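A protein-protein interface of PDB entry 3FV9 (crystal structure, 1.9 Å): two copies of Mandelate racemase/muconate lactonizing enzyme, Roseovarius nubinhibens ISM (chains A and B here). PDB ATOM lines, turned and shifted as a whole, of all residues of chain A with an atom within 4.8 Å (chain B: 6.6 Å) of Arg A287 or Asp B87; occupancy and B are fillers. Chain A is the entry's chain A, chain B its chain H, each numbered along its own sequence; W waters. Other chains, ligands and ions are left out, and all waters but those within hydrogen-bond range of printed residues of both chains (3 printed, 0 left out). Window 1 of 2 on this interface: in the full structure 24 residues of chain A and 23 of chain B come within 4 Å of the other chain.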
ATOM      1  N   THR A 127     -15.420   9.473 -13.494  1.00  0.00           N
ATOM      2  CA  THR A 127     -15.995  10.792 -13.786  1.00  0.00           C
ATOM      3  C   THR A 127     -15.121  11.558 -14.784  1.00  0.00           C
ATOM      4  O   THR A 127     -14.965  12.773 -14.688  1.00  0.00           O
ATOM      5  CB  THR A 127     -16.227  11.615 -12.490  1.00  0.00           C
ATOM      6  OG1 THR A 127     -14.988  11.742 -11.773  1.00  0.00           O
ATOM      7  CG2 THR A 127     -17.267  10.932 -11.589  1.00  0.00           C
ATOM      8  N   GLY A 128     -14.545  10.826 -15.739  1.00  0.00           N
ATOM      9  CA  GLY A 128     -13.791  11.432 -16.834  1.00  0.00           C
ATOM     10  C   GLY A 128     -12.346  10.958 -16.929  1.00  0.00           C
ATOM     11  O   GLY A 128     -11.787  10.870 -18.024  1.00  0.00           O
ATOM     12  N   LEU A 272     -18.715  25.512  -6.901  1.00  0.00           N
ATOM     13  CA  LEU A 272     -19.499  24.273  -6.914  1.00  0.00           C
ATOM     14  C   LEU A 272     -19.265  23.494  -5.632  1.00  0.00           C
ATOM     15  O   LEU A 272     -18.125  23.117  -5.337  1.00  0.00           O
ATOM     16  CB  LEU A 272     -19.153  23.415  -8.132  1.00  0.00           C
ATOM     17  CG  LEU A 272     -19.462  24.004  -9.508  1.00  0.00           C
ATOM     18  CD1 LEU A 272     -18.977  23.061 -10.595  1.00  0.00           C
ATOM     19  CD2 LEU A 272     -20.952  24.299  -9.659  1.00  0.00           C
ATOM     20  N   PRO A 282     -25.449  16.042 -10.266  1.00  0.00           N
ATOM     21  CA  PRO A 282     -25.491  17.452 -10.716  1.00  0.00           C
ATOM     22  C   PRO A 282     -24.144  18.179 -10.714  1.00  0.00           C
ATOM     23  O   PRO A 282     -23.975  19.144 -11.456  1.00  0.00           O
ATOM     24  CB  PRO A 282     -26.424  18.110  -9.709  1.00  0.00           C
ATOM     25  CG  PRO A 282     -26.385  17.206  -8.502  1.00  0.00           C
ATOM     26  CD  PRO A 282     -26.215  15.832  -9.021  1.00  0.00           C
ATOM     27  N   MET A 283     -23.194  17.751  -9.878  1.00  0.00           N
ATOM     28  CA  MET A 283     -21.831  18.299  -9.976  1.00  0.00           C
ATOM     29  C   MET A 283     -21.276  18.081 -11.390  1.00  0.00           C
ATOM     30  O   MET A 283     -20.623  18.959 -11.954  1.00  0.00           O
ATOM     31  CB  MET A 283     -20.888  17.668  -8.916  1.00  0.00           C
ATOM     32  CG  MET A 283     -21.031  18.281  -7.506  1.00  0.00           C
ATOM     33  SD  MET A 283     -20.460  20.000  -7.317  1.00  0.00           S
ATOM     34  CE  MET A 283     -18.686  19.742  -7.460  1.00  0.00           C
ATOM     35  N   LEU A 284     -21.563  16.916 -11.963  1.00  0.00           N
ATOM     36  CA  LEU A 284     -21.080  16.579 -13.310  1.00  0.00           C
ATOM     37  C   LEU A 284     -21.802  17.361 -14.399  1.00  0.00           C
ATOM     38  O   LEU A 284     -21.172  17.833 -15.350  1.00  0.00           O
ATOM     39  CB  LEU A 284     -21.202  15.071 -13.575  1.00  0.00           C
ATOM     40  CG  LEU A 284     -20.261  14.162 -12.775  1.00  0.00           C
ATOM     41  CD1 LEU A 284     -20.576  12.694 -13.091  1.00  0.00           C
ATOM     42  CD2 LEU A 284     -18.810  14.472 -13.102  1.00  0.00           C
ATOM     43  N   ARG A 285     -23.124  17.480 -14.264  1.00  0.00           N
ATOM     44  CA  ARG A 285     -23.923  18.295 -15.187  1.00  0.00           C
ATOM     45  C   ARG A 285     -23.461  19.753 -15.152  1.00  0.00           C
ATOM     46  O   ARG A 285     -23.312  20.407 -16.195  1.00  0.00           O
ATOM     47  CB  ARG A 285     -25.415  18.214 -14.827  1.00  0.00           C
ATOM     48  CG  ARG A 285     -26.032  16.815 -14.934  1.00  0.00           C
ATOM     49  CD  ARG A 285     -27.467  16.802 -14.414  1.00  0.00           C
ATOM     50  NE  ARG A 285     -28.040  15.458 -14.489  1.00  0.00           N
ATOM     51  CZ  ARG A 285     -29.336  15.182 -14.371  1.00  0.00           C
ATOM     52  NH1 ARG A 285     -30.221  16.157 -14.178  1.00  0.00           N
ATOM     53  NH2 ARG A 285     -29.749  13.927 -14.459  1.00  0.00           N
ATOM     54  N   GLN A 286     -23.242  20.268 -13.950  1.00  0.00           N
ATOM     55  CA  GLN A 286     -22.876  21.669 -13.791  1.00  0.00           C
ATOM     56  C   GLN A 286     -21.442  21.948 -14.213  1.00  0.00           C
ATOM     57  O   GLN A 286     -21.158  23.004 -14.794  1.00  0.00           O
ATOM     58  CB  GLN A 286     -23.204  22.147 -12.379  1.00  0.00           C
ATOM     59  CG  GLN A 286     -24.743  22.150 -12.149  1.00  0.00           C
ATOM     60  CD  GLN A 286     -25.145  22.516 -10.733  1.00  0.00           C
ATOM     61  OE1 GLN A 286     -24.437  23.258 -10.051  1.00  0.00           O
ATOM     62  NE2 GLN A 286     -26.287  21.989 -10.281  1.00  0.00           N
ATOM     63  N   ARG A 287     -20.555  20.978 -13.989  1.00  0.00           N
ATOM     64  CA  ARG A 287     -19.197  21.062 -14.529  1.00  0.00           C
ATOM     65  C   ARG A 287     -19.204  21.094 -16.063  1.00  0.00           C
ATOM     66  O   ARG A 287     -18.451  21.839 -16.677  1.00  0.00           O
ATOM     67  CB  ARG A 287     -18.346  19.894 -14.018  1.00  0.00           C
ATOM     68  CG  ARG A 287     -16.887  19.948 -14.447  1.00  0.00           C
ATOM     69  CD  ARG A 287     -16.094  18.893 -13.690  1.00  0.00           C
ATOM     70  NE  ARG A 287     -16.225  17.587 -14.319  1.00  0.00           N
ATOM     71  CZ  ARG A 287     -15.634  16.483 -13.880  1.00  0.00           C
ATOM     72  NH1 ARG A 287     -15.809  15.353 -14.536  1.00  0.00           N
ATOM     73  NH2 ARG A 287     -14.864  16.514 -12.802  1.00  0.00           N
ATOM     74  N   ALA A 288     -20.055  20.279 -16.680  1.00  0.00           N
ATOM     75  CA  ALA A 288     -20.156  20.262 -18.148  1.00  0.00           C
ATOM     76  C   ALA A 288     -20.654  21.620 -18.676  1.00  0.00           C
ATOM     77  O   ALA A 288     -20.179  22.123 -19.706  1.00  0.00           O
ATOM     78  CB  ALA A 288     -21.084  19.145 -18.596  1.00  0.00           C
ATOM     79  N   ILE A 289     -21.624  22.202 -17.980  1.00  0.00           N
ATOM     80  CA  ILE A 289     -22.157  23.503 -18.399  1.00  0.00           C
ATOM     81  C   ILE A 289     -21.101  24.600 -18.220  1.00  0.00           C
ATOM     82  O   ILE A 289     -20.810  25.366 -19.140  1.00  0.00           O
ATOM     83  CB  ILE A 289     -23.457  23.846 -17.629  1.00  0.00           C
ATOM     84  CG1 ILE A 289     -24.541  22.800 -17.959  1.00  0.00           C
ATOM     85  CG2 ILE A 289     -23.895  25.292 -17.956  1.00  0.00           C
ATOM     86  CD1 ILE A 289     -25.771  22.790 -17.005  1.00  0.00           C
ATOM     87  N   ALA A 290     -20.529  24.665 -17.026  1.00  0.00           N
ATOM     88  CA  ALA A 290     -19.506  25.665 -16.712  1.00  0.00           C
ATOM     89  C   ALA A 290     -18.317  25.564 -17.666  1.00  0.00           C
ATOM     90  O   ALA A 290     -17.878  26.575 -18.224  1.00  0.00           O
ATOM     91  CB  ALA A 290     -19.042  25.503 -15.246  1.00  0.00           C
ATOM     92  N   ALA A 291     -17.813  24.343 -17.867  1.00  0.00           N
ATOM     93  CA  ALA A 291     -16.674  24.104 -18.757  1.00  0.00           C
ATOM     94  C   ALA A 291     -16.952  24.607 -20.166  1.00  0.00           C
ATOM     95  O   ALA A 291     -16.101  25.260 -20.779  1.00  0.00           O
ATOM     96  CB  ALA A 291     -16.273  22.609 -18.779  1.00  0.00           C
ATOM     97  N   ALA A 292     -18.147  24.316 -20.665  1.00  0.00           N
ATOM     98  CA  ALA A 292     -18.546  24.772 -21.990  1.00  0.00           C
ATOM     99  C   ALA A 292     -18.577  26.295 -22.058  1.00  0.00           C
ATOM    100  O   ALA A 292     -18.218  26.873 -23.084  1.00  0.00           O
ATOM    101  CB  ALA A 292     -19.905  24.196 -22.357  1.00  0.00           C
ATOM    102  N   MET A 297     -13.975  27.048 -11.882  1.00  0.00           N
ATOM    103  CA  MET A 297     -14.780  26.324 -10.904  1.00  0.00           C
ATOM    104  C   MET A 297     -13.941  26.089  -9.657  1.00  0.00           C
ATOM    105  O   MET A 297     -12.866  25.497  -9.749  1.00  0.00           O
ATOM    106  CB  MET A 297     -15.160  24.940 -11.456  1.00  0.00           C
ATOM    107  CG  MET A 297     -16.248  24.869 -12.530  1.00  0.00           C
ATOM    108  SD  MET A 297     -16.231  23.219 -13.279  1.00  0.00           S
ATOM    109  CE  MET A 297     -15.344  23.595 -14.789  1.00  0.00           C
ATOM    110  N   LEU A 315     -13.917  14.440  -7.606  1.00  0.00           N
ATOM    111  CA  LEU A 315     -14.429  15.376  -8.613  1.00  0.00           C
ATOM    112  C   LEU A 315     -13.383  16.411  -9.021  1.00  0.00           C
ATOM    113  O   LEU A 315     -13.177  16.669 -10.220  1.00  0.00           O
ATOM    114  CB  LEU A 315     -15.689  16.062  -8.088  1.00  0.00           C
ATOM    115  CG  LEU A 315     -16.917  15.152  -8.066  1.00  0.00           C
ATOM    116  CD1 LEU A 315     -18.031  15.831  -7.283  1.00  0.00           C
ATOM    117  CD2 LEU A 315     -17.371  14.814  -9.490  1.00  0.00           C
ATOM    118  N   SER A 318     -10.749  15.000 -11.445  1.00  0.00           N
ATOM    119  CA  SER A 318     -11.141  14.784 -12.842  1.00  0.00           C
ATOM    120  C   SER A 318     -11.558  16.079 -13.560  1.00  0.00           C
ATOM    121  O   SER A 318     -11.997  16.045 -14.708  1.00  0.00           O
ATOM    122  CB  SER A 318     -12.260  13.749 -12.928  1.00  0.00           C
ATOM    123  OG  SER A 318     -13.378  14.155 -12.164  1.00  0.00           O
ATOM    124  N   THR A 319     -11.415  17.215 -12.883  1.00  0.00           N
ATOM    125  CA  THR A 319     -11.706  18.523 -13.483  1.00  0.00           C
ATOM    126  C   THR A 319     -10.484  19.035 -14.276  1.00  0.00           C
ATOM    127  O   THR A 319      -9.364  18.965 -13.778  1.00  0.00           O
ATOM    128  CB  THR A 319     -12.146  19.506 -12.360  1.00  0.00           C
ATOM    129  OG1 THR A 319     -13.269  18.943 -11.678  1.00  0.00           O
ATOM    130  CG2 THR A 319     -12.549  20.881 -12.883  1.00  0.00           C
ATOM    131  N   ARG B  84     -11.806   3.790 -20.826  1.00  0.00           N
ATOM    132  CA  ARG B  84     -12.860   4.171 -19.899  1.00  0.00           C
ATOM    133  C   ARG B  84     -12.785   5.647 -19.500  1.00  0.00           C
ATOM    134  O   ARG B  84     -13.738   6.180 -18.951  1.00  0.00           O
ATOM    135  CB  ARG B  84     -12.840   3.276 -18.651  1.00  0.00           C
ATOM    136  CG  ARG B  84     -13.147   1.803 -18.936  1.00  0.00           C
ATOM    137  CD  ARG B  84     -12.857   0.888 -17.732  1.00  0.00           C
ATOM    138  NE  ARG B  84     -11.446   0.931 -17.345  1.00  0.00           N
ATOM    139  CZ  ARG B  84     -10.913   0.239 -16.346  1.00  0.00           C
ATOM    140  NH1 ARG B  84     -11.669  -0.572 -15.604  1.00  0.00           N
ATOM    141  NH2 ARG B  84      -9.616   0.363 -16.090  1.00  0.00           N
ATOM    142  N   GLN B  85     -11.651   6.295 -19.764  1.00  0.00           N
ATOM    143  CA  GLN B  85     -11.417   7.665 -19.303  1.00  0.00           C
ATOM    144  C   GLN B  85     -11.787   8.634 -20.422  1.00  0.00           C
ATOM    145  O   GLN B  85     -10.938   9.262 -21.048  1.00  0.00           O
ATOM    146  CB  GLN B  85      -9.979   7.835 -18.806  1.00  0.00           C
ATOM    147  CG  GLN B  85      -9.707   7.026 -17.521  1.00  0.00           C
ATOM    148  CD  GLN B  85      -8.313   7.230 -16.938  1.00  0.00           C
ATOM    149  OE1 GLN B  85      -7.796   6.357 -16.224  1.00  0.00           O
ATOM    150  NE2 GLN B  85      -7.703   8.373 -17.221  1.00  0.00           N
ATOM    151  N   HIS B  86     -13.089   8.739 -20.650  1.00  0.00           N
ATOM    152  CA  HIS B  86     -13.628   9.445 -21.820  1.00  0.00           C
ATOM    153  C   HIS B  86     -13.189  10.901 -21.936  1.00  0.00           C
ATOM    154  O   HIS B  86     -12.937  11.392 -23.038  1.00  0.00           O
ATOM    155  CB  HIS B  86     -15.161   9.333 -21.893  1.00  0.00           C
ATOM    156  CG  HIS B  86     -15.866   9.654 -20.611  1.00  0.00           C
ATOM    157  ND1 HIS B  86     -16.330   8.680 -19.754  1.00  0.00           N
ATOM    158  CD2 HIS B  86     -16.214  10.839 -20.054  1.00  0.00           C
ATOM    159  CE1 HIS B  86     -16.919   9.251 -18.719  1.00  0.00           C
ATOM    160  NE2 HIS B  86     -16.861  10.560 -18.874  1.00  0.00           N
ATOM    161  N   ASP B  87     -13.097  11.603 -20.803  1.00  0.00           N
ATOM    162  CA  ASP B  87     -12.703  13.016 -20.833  1.00  0.00           C
ATOM    163  C   ASP B  87     -11.214  13.189 -21.148  1.00  0.00           C
ATOM    164  O   ASP B  87     -10.826  14.117 -21.847  1.00  0.00           O
ATOM    165  CB  ASP B  87     -13.040  13.731 -19.518  1.00  0.00           C
ATOM    166  CG  ASP B  87     -14.536  13.961 -19.320  1.00  0.00           C
ATOM    167  OD1 ASP B  87     -14.899  14.425 -18.217  1.00  0.00           O
ATOM    168  OD2 ASP B  87     -15.345  13.704 -20.245  1.00  0.00           O
ATOM    169  N   ARG B  88     -10.381  12.289 -20.632  1.00  0.00           N
ATOM    170  CA  ARG B  88      -8.945  12.393 -20.863  1.00  0.00           C
ATOM    171  C   ARG B  88      -8.588  11.971 -22.291  1.00  0.00           C
ATOM    172  O   ARG B  88      -7.691  12.559 -22.907  1.00  0.00           O
ATOM    173  CB  ARG B  88      -8.147  11.617 -19.804  1.00  0.00           C
ATOM    174  CG  ARG B  88      -8.465  12.007 -18.342  1.00  0.00           C
ATOM    175  CD  ARG B  88      -7.984  13.413 -17.922  1.00  0.00           C
ATOM    176  NE  ARG B  88      -8.828  14.521 -18.407  1.00  0.00           N
ATOM    177  CZ  ARG B  88      -9.967  14.928 -17.845  1.00  0.00           C
ATOM    178  NH1 ARG B  88     -10.447  14.316 -16.765  1.00  0.00           N
ATOM    179  NH2 ARG B  88     -10.632  15.966 -18.358  1.00  0.00           N
ATOM    180  N   ILE B  89      -9.296  10.964 -22.809  1.00  0.00           N
ATOM    181  CA  ILE B  89      -9.182  10.589 -24.225  1.00  0.00           C
ATOM    182  C   ILE B  89      -9.661  11.756 -25.114  1.00  0.00           C
ATOM    183  O   ILE B  89      -9.041  12.061 -26.143  1.00  0.00           O
ATOM    184  CB  ILE B  89     -10.002   9.328 -24.553  1.00  0.00           C
ATOM    185  CG1 ILE B  89      -9.432   8.112 -23.823  1.00  0.00           C
ATOM    186  CG2 ILE B  89     -10.034   9.071 -26.080  1.00  0.00           C
ATOM    187  CD1 ILE B  89     -10.354   6.911 -23.880  1.00  0.00           C
ATOM    188  N   TRP B  90     -10.755  12.400 -24.710  1.00  0.00           N
ATOM    189  CA  TRP B  90     -11.264  13.583 -25.428  1.00  0.00           C
ATOM    190  C   TRP B  90     -10.223  14.701 -25.484  1.00  0.00           C
ATOM    191  O   TRP B  90      -9.974  15.269 -26.543  1.00  0.00           O
ATOM    192  CB  TRP B  90     -12.567  14.085 -24.797  1.00  0.00           C
ATOM    193  CG  TRP B  90     -13.259  15.197 -25.580  1.00  0.00           C
ATOM    194  CD1 TRP B  90     -13.281  16.519 -25.272  1.00  0.00           C
ATOM    195  CD2 TRP B  90     -14.032  15.052 -26.779  1.00  0.00           C
ATOM    196  NE1 TRP B  90     -14.010  17.218 -26.209  1.00  0.00           N
ATOM    197  CE2 TRP B  90     -14.481  16.338 -27.145  1.00  0.00           C
ATOM    198  CE3 TRP B  90     -14.381  13.961 -27.582  1.00  0.00           C
ATOM    199  CZ2 TRP B  90     -15.276  16.559 -28.279  1.00  0.00           C
ATOM    200  CZ3 TRP B  90     -15.155  14.187 -28.713  1.00  0.00           C
ATOM    201  CH2 TRP B  90     -15.587  15.471 -29.050  1.00  0.00           C
ATOM    202  N   ASP B  91      -9.619  15.002 -24.338  1.00  0.00           N
ATOM    203  CA  ASP B  91      -8.559  16.002 -24.243  1.00  0.00           C
ATOM    204  C   ASP B  91      -7.354  15.666 -25.126  1.00  0.00           C
ATOM    205  O   ASP B  91      -6.812  16.546 -25.787  1.00  0.00           O
ATOM    206  CB  ASP B  91      -8.094  16.149 -22.787  1.00  0.00           C
ATOM    207  CG  ASP B  91      -9.106  16.869 -21.911  1.00  0.00           C
ATOM    208  OD1 ASP B  91      -8.927  16.830 -20.678  1.00  0.00           O
ATOM    209  OD2 ASP B  91     -10.079  17.461 -22.428  1.00  0.00           O
ATOM    210  N   ARG B  92      -6.926  14.401 -25.111  1.00  0.00           N
ATOM    211  CA  ARG B  92      -5.851  13.943 -25.989  1.00  0.00           C
ATOM    212  C   ARG B  92      -6.170  14.263 -27.457  1.00  0.00           C
ATOM    213  O   ARG B  92      -5.351  14.855 -28.161  1.00  0.00           O
ATOM    214  CB  ARG B  92      -5.602  12.441 -25.807  1.00  0.00           C
ATOM    215  CG  ARG B  92      -4.483  11.865 -26.690  1.00  0.00           C
ATOM    216  CD  ARG B  92      -3.099  12.416 -26.342  1.00  0.00           C
ATOM    217  NE  ARG B  92      -2.693  12.136 -24.962  1.00  0.00           N
ATOM    218  CZ  ARG B  92      -2.136  11.000 -24.539  1.00  0.00           C
ATOM    219  NH1 ARG B  92      -1.803  10.871 -23.259  1.00  0.00           N
ATOM    220  NH2 ARG B  92      -1.909   9.987 -25.377  1.00  0.00           N
ATOM    221  N   ASP B 108     -14.317   7.798 -30.288  1.00  0.00           N
ATOM    222  CA  ASP B 108     -15.011   8.027 -29.033  1.00  0.00           C
ATOM    223  C   ASP B 108     -16.098   6.980 -28.766  1.00  0.00           C
ATOM    224  O   ASP B 108     -16.234   6.496 -27.633  1.00  0.00           O
ATOM    225  CB  ASP B 108     -15.611   9.430 -28.991  1.00  0.00           C
ATOM    226  CG  ASP B 108     -16.271   9.727 -27.667  1.00  0.00           C
ATOM    227  OD1 ASP B 108     -15.554  10.061 -26.703  1.00  0.00           O
ATOM    228  OD2 ASP B 108     -17.502   9.606 -27.580  1.00  0.00           O
ATOM    229  N   TRP B 112     -16.557   4.046 -25.736  1.00  0.00           N
ATOM    230  CA  TRP B 112     -17.761   3.895 -24.916  1.00  0.00           C
ATOM    231  C   TRP B 112     -18.345   2.484 -25.019  1.00  0.00           C
ATOM    232  O   TRP B 112     -18.850   1.941 -24.030  1.00  0.00           O
ATOM    233  CB  TRP B 112     -18.811   4.934 -25.300  1.00  0.00           C
ATOM    234  CG  TRP B 112     -18.633   6.250 -24.595  1.00  0.00           C
ATOM    235  CD1 TRP B 112     -17.988   7.356 -25.071  1.00  0.00           C
ATOM    236  CD2 TRP B 112     -19.109   6.593 -23.290  1.00  0.00           C
ATOM    237  NE1 TRP B 112     -18.034   8.372 -24.145  1.00  0.00           N
ATOM    238  CE2 TRP B 112     -18.724   7.933 -23.043  1.00  0.00           C
ATOM    239  CE3 TRP B 112     -19.836   5.903 -22.307  1.00  0.00           C
ATOM    240  CZ2 TRP B 112     -19.042   8.599 -21.850  1.00  0.00           C
ATOM    241  CZ3 TRP B 112     -20.151   6.566 -21.119  1.00  0.00           C
ATOM    242  CH2 TRP B 112     -19.747   7.902 -20.902  1.00  0.00           C
ATOM    243  N   THR B 281     -19.310  11.122 -25.821  1.00  0.00           N
ATOM    244  CA  THR B 281     -18.836  12.132 -24.859  1.00  0.00           C
ATOM    245  C   THR B 281     -19.458  13.526 -25.074  1.00  0.00           C
ATOM    246  O   THR B 281     -20.093  14.068 -24.155  1.00  0.00           O
ATOM    247  CB  THR B 281     -17.282  12.183 -24.815  1.00  0.00           C
ATOM    248  OG1 THR B 281     -16.791  10.863 -24.578  1.00  0.00           O
ATOM    249  CG2 THR B 281     -16.797  13.079 -23.680  1.00  0.00           C
ATOM    250  N   ARG B 285     -22.371  15.723 -22.968  1.00  0.00           N
ATOM    251  CA  ARG B 285     -22.143  17.114 -22.545  1.00  0.00           C
ATOM    252  C   ARG B 285     -23.235  18.037 -23.077  1.00  0.00           C
ATOM    253  O   ARG B 285     -23.816  18.825 -22.329  1.00  0.00           O
ATOM    254  CB  ARG B 285     -20.768  17.617 -23.007  1.00  0.00           C
ATOM    255  CG  ARG B 285     -19.598  16.898 -22.377  1.00  0.00           C
ATOM    256  CD  ARG B 285     -18.285  17.435 -22.940  1.00  0.00           C
ATOM    257  NE  ARG B 285     -17.155  16.653 -22.446  1.00  0.00           N
ATOM    258  CZ  ARG B 285     -15.881  17.000 -22.597  1.00  0.00           C
ATOM    259  NH1 ARG B 285     -15.565  18.125 -23.234  1.00  0.00           N
ATOM    260  NH2 ARG B 285     -14.923  16.220 -22.108  1.00  0.00           N
HETATM  261  O   HOH W   1     -14.256   8.283 -16.788  1.00  0.00           O
HETATM  262  O   HOH W   2     -17.109  14.549 -16.874  1.00  0.00           O
HETATM  263  O   HOH W   3     -13.327  16.306 -17.181  1.00  0.00           O
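Asp B87 touches Thr A127 (OD1 to O, 3.9 Å). Gly A128 touches Gln B85 (O to C, 3.3 Å). O of Gly A128 touches N of His B86 (3.6 Å).
The side-chain hydroxyl of Thr A127 lies within hydrogen-bond range of the side-chain hydroxyl of Ser A318 (2.9 Å). The guanidinium group (NH2) of Arg A287 is in hydrogen-bond range of the backbone carbonyl oxygen (O) of Leu A315 (3.1 Å). NH2 of Arg A287 lies within hydrogen-bond range of OG of Ser A318, at 2.9 Å. NH2 of Arg A287 lies within hydrogen-bond range of OG1 of Thr A319, 3.1 Å away. OG of Ser A318 sits at hydrogen-bond distance from O of Leu A315 (3.2 Å). OD1 of Asp B91 is in salt-bridge range of NH2 of Arg B88 (3.0 Å).
Water W2 bridges OD1 of Asp B87 and NH1 of Arg A287. Water W3 lies within hydrogen-bond range of the side-chain carboxylate (OD1) of Asp B87 (2.7 Å), the backbone carbonyl oxygen (O) of Ser A318 (2.8 Å) and the guanidinium group (NH2) of Arg B88 (3.0 Å). Water W1 bridges N of Gly A128 (2.8 Å) and O of Arg B84 (3.1 Å).
Position printed for both chains: 285. Of the 7 pairs that touch across the chains among the printed residues, none has its exchanged pair printed and touching as well.
Of the 18 printed residues of chain A, 4 touch a printed residue of chain B. Printed residues of chain A that touch a printed residue of chain B: Thr A127, Gly A128, Arg A287 and Ser A318. Of the 13 printed residues of chain B, 4 touch a printed residue of chain A. Hydrophobic or aromatic side chains of chain B within 4 Å of the printed part of chain A: His B86. Among the printed residues, 7 pairs touch across the chains. Among the printed residues, Asp or Glu carboxylates within 4 Å of a Lys or Arg side-chain nitrogen of the other chain: Arg A287 with Asp B87.
Printed residues of chain B within 4 Å of Thr A127: Asp B87. Of the printed residues of chain B, Gly A128 touches Gln B85 (3.3 Å), His B86 (3.6 Å), Asp B87 (3.2 Å) and Arg B88 (3.3 Å). Leu A284 touches none of the printed residues of chain B. Arg A287 touches just one residue of chain B: Asp B87. Of the printed residues of chain B, Ser A318 touches Arg B88 (3.1 Å). Arg B84 touches none of the printed residues of chain A. Printed residues of chain A within 4 Å of Gln B85: Gly A128. Printed residues of chain A within 4 Å of His B86: Gly A128 (3.6 Å). The nearest printed residue of chain A that does not touch Asp B87 is Ser A318 (4.8 Å).
O of Gly A128 sits at hydrogen-bond distance from N of Asp B87, 3.2 Å away. The backbone carbonyl oxygen (O) of Gly A128 sits at hydrogen-bond distance from the backbone NH (N) of Arg B88 (3.3 Å). NH1 of Arg A287 is in salt-bridge range of OD1 of Asp B87 (3.9 Å). The guanidinium group (NH1) of Arg B88 is in hydrogen-bond range of the backbone carbonyl oxygen (O) of Ser A318, 3.1 Å away.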
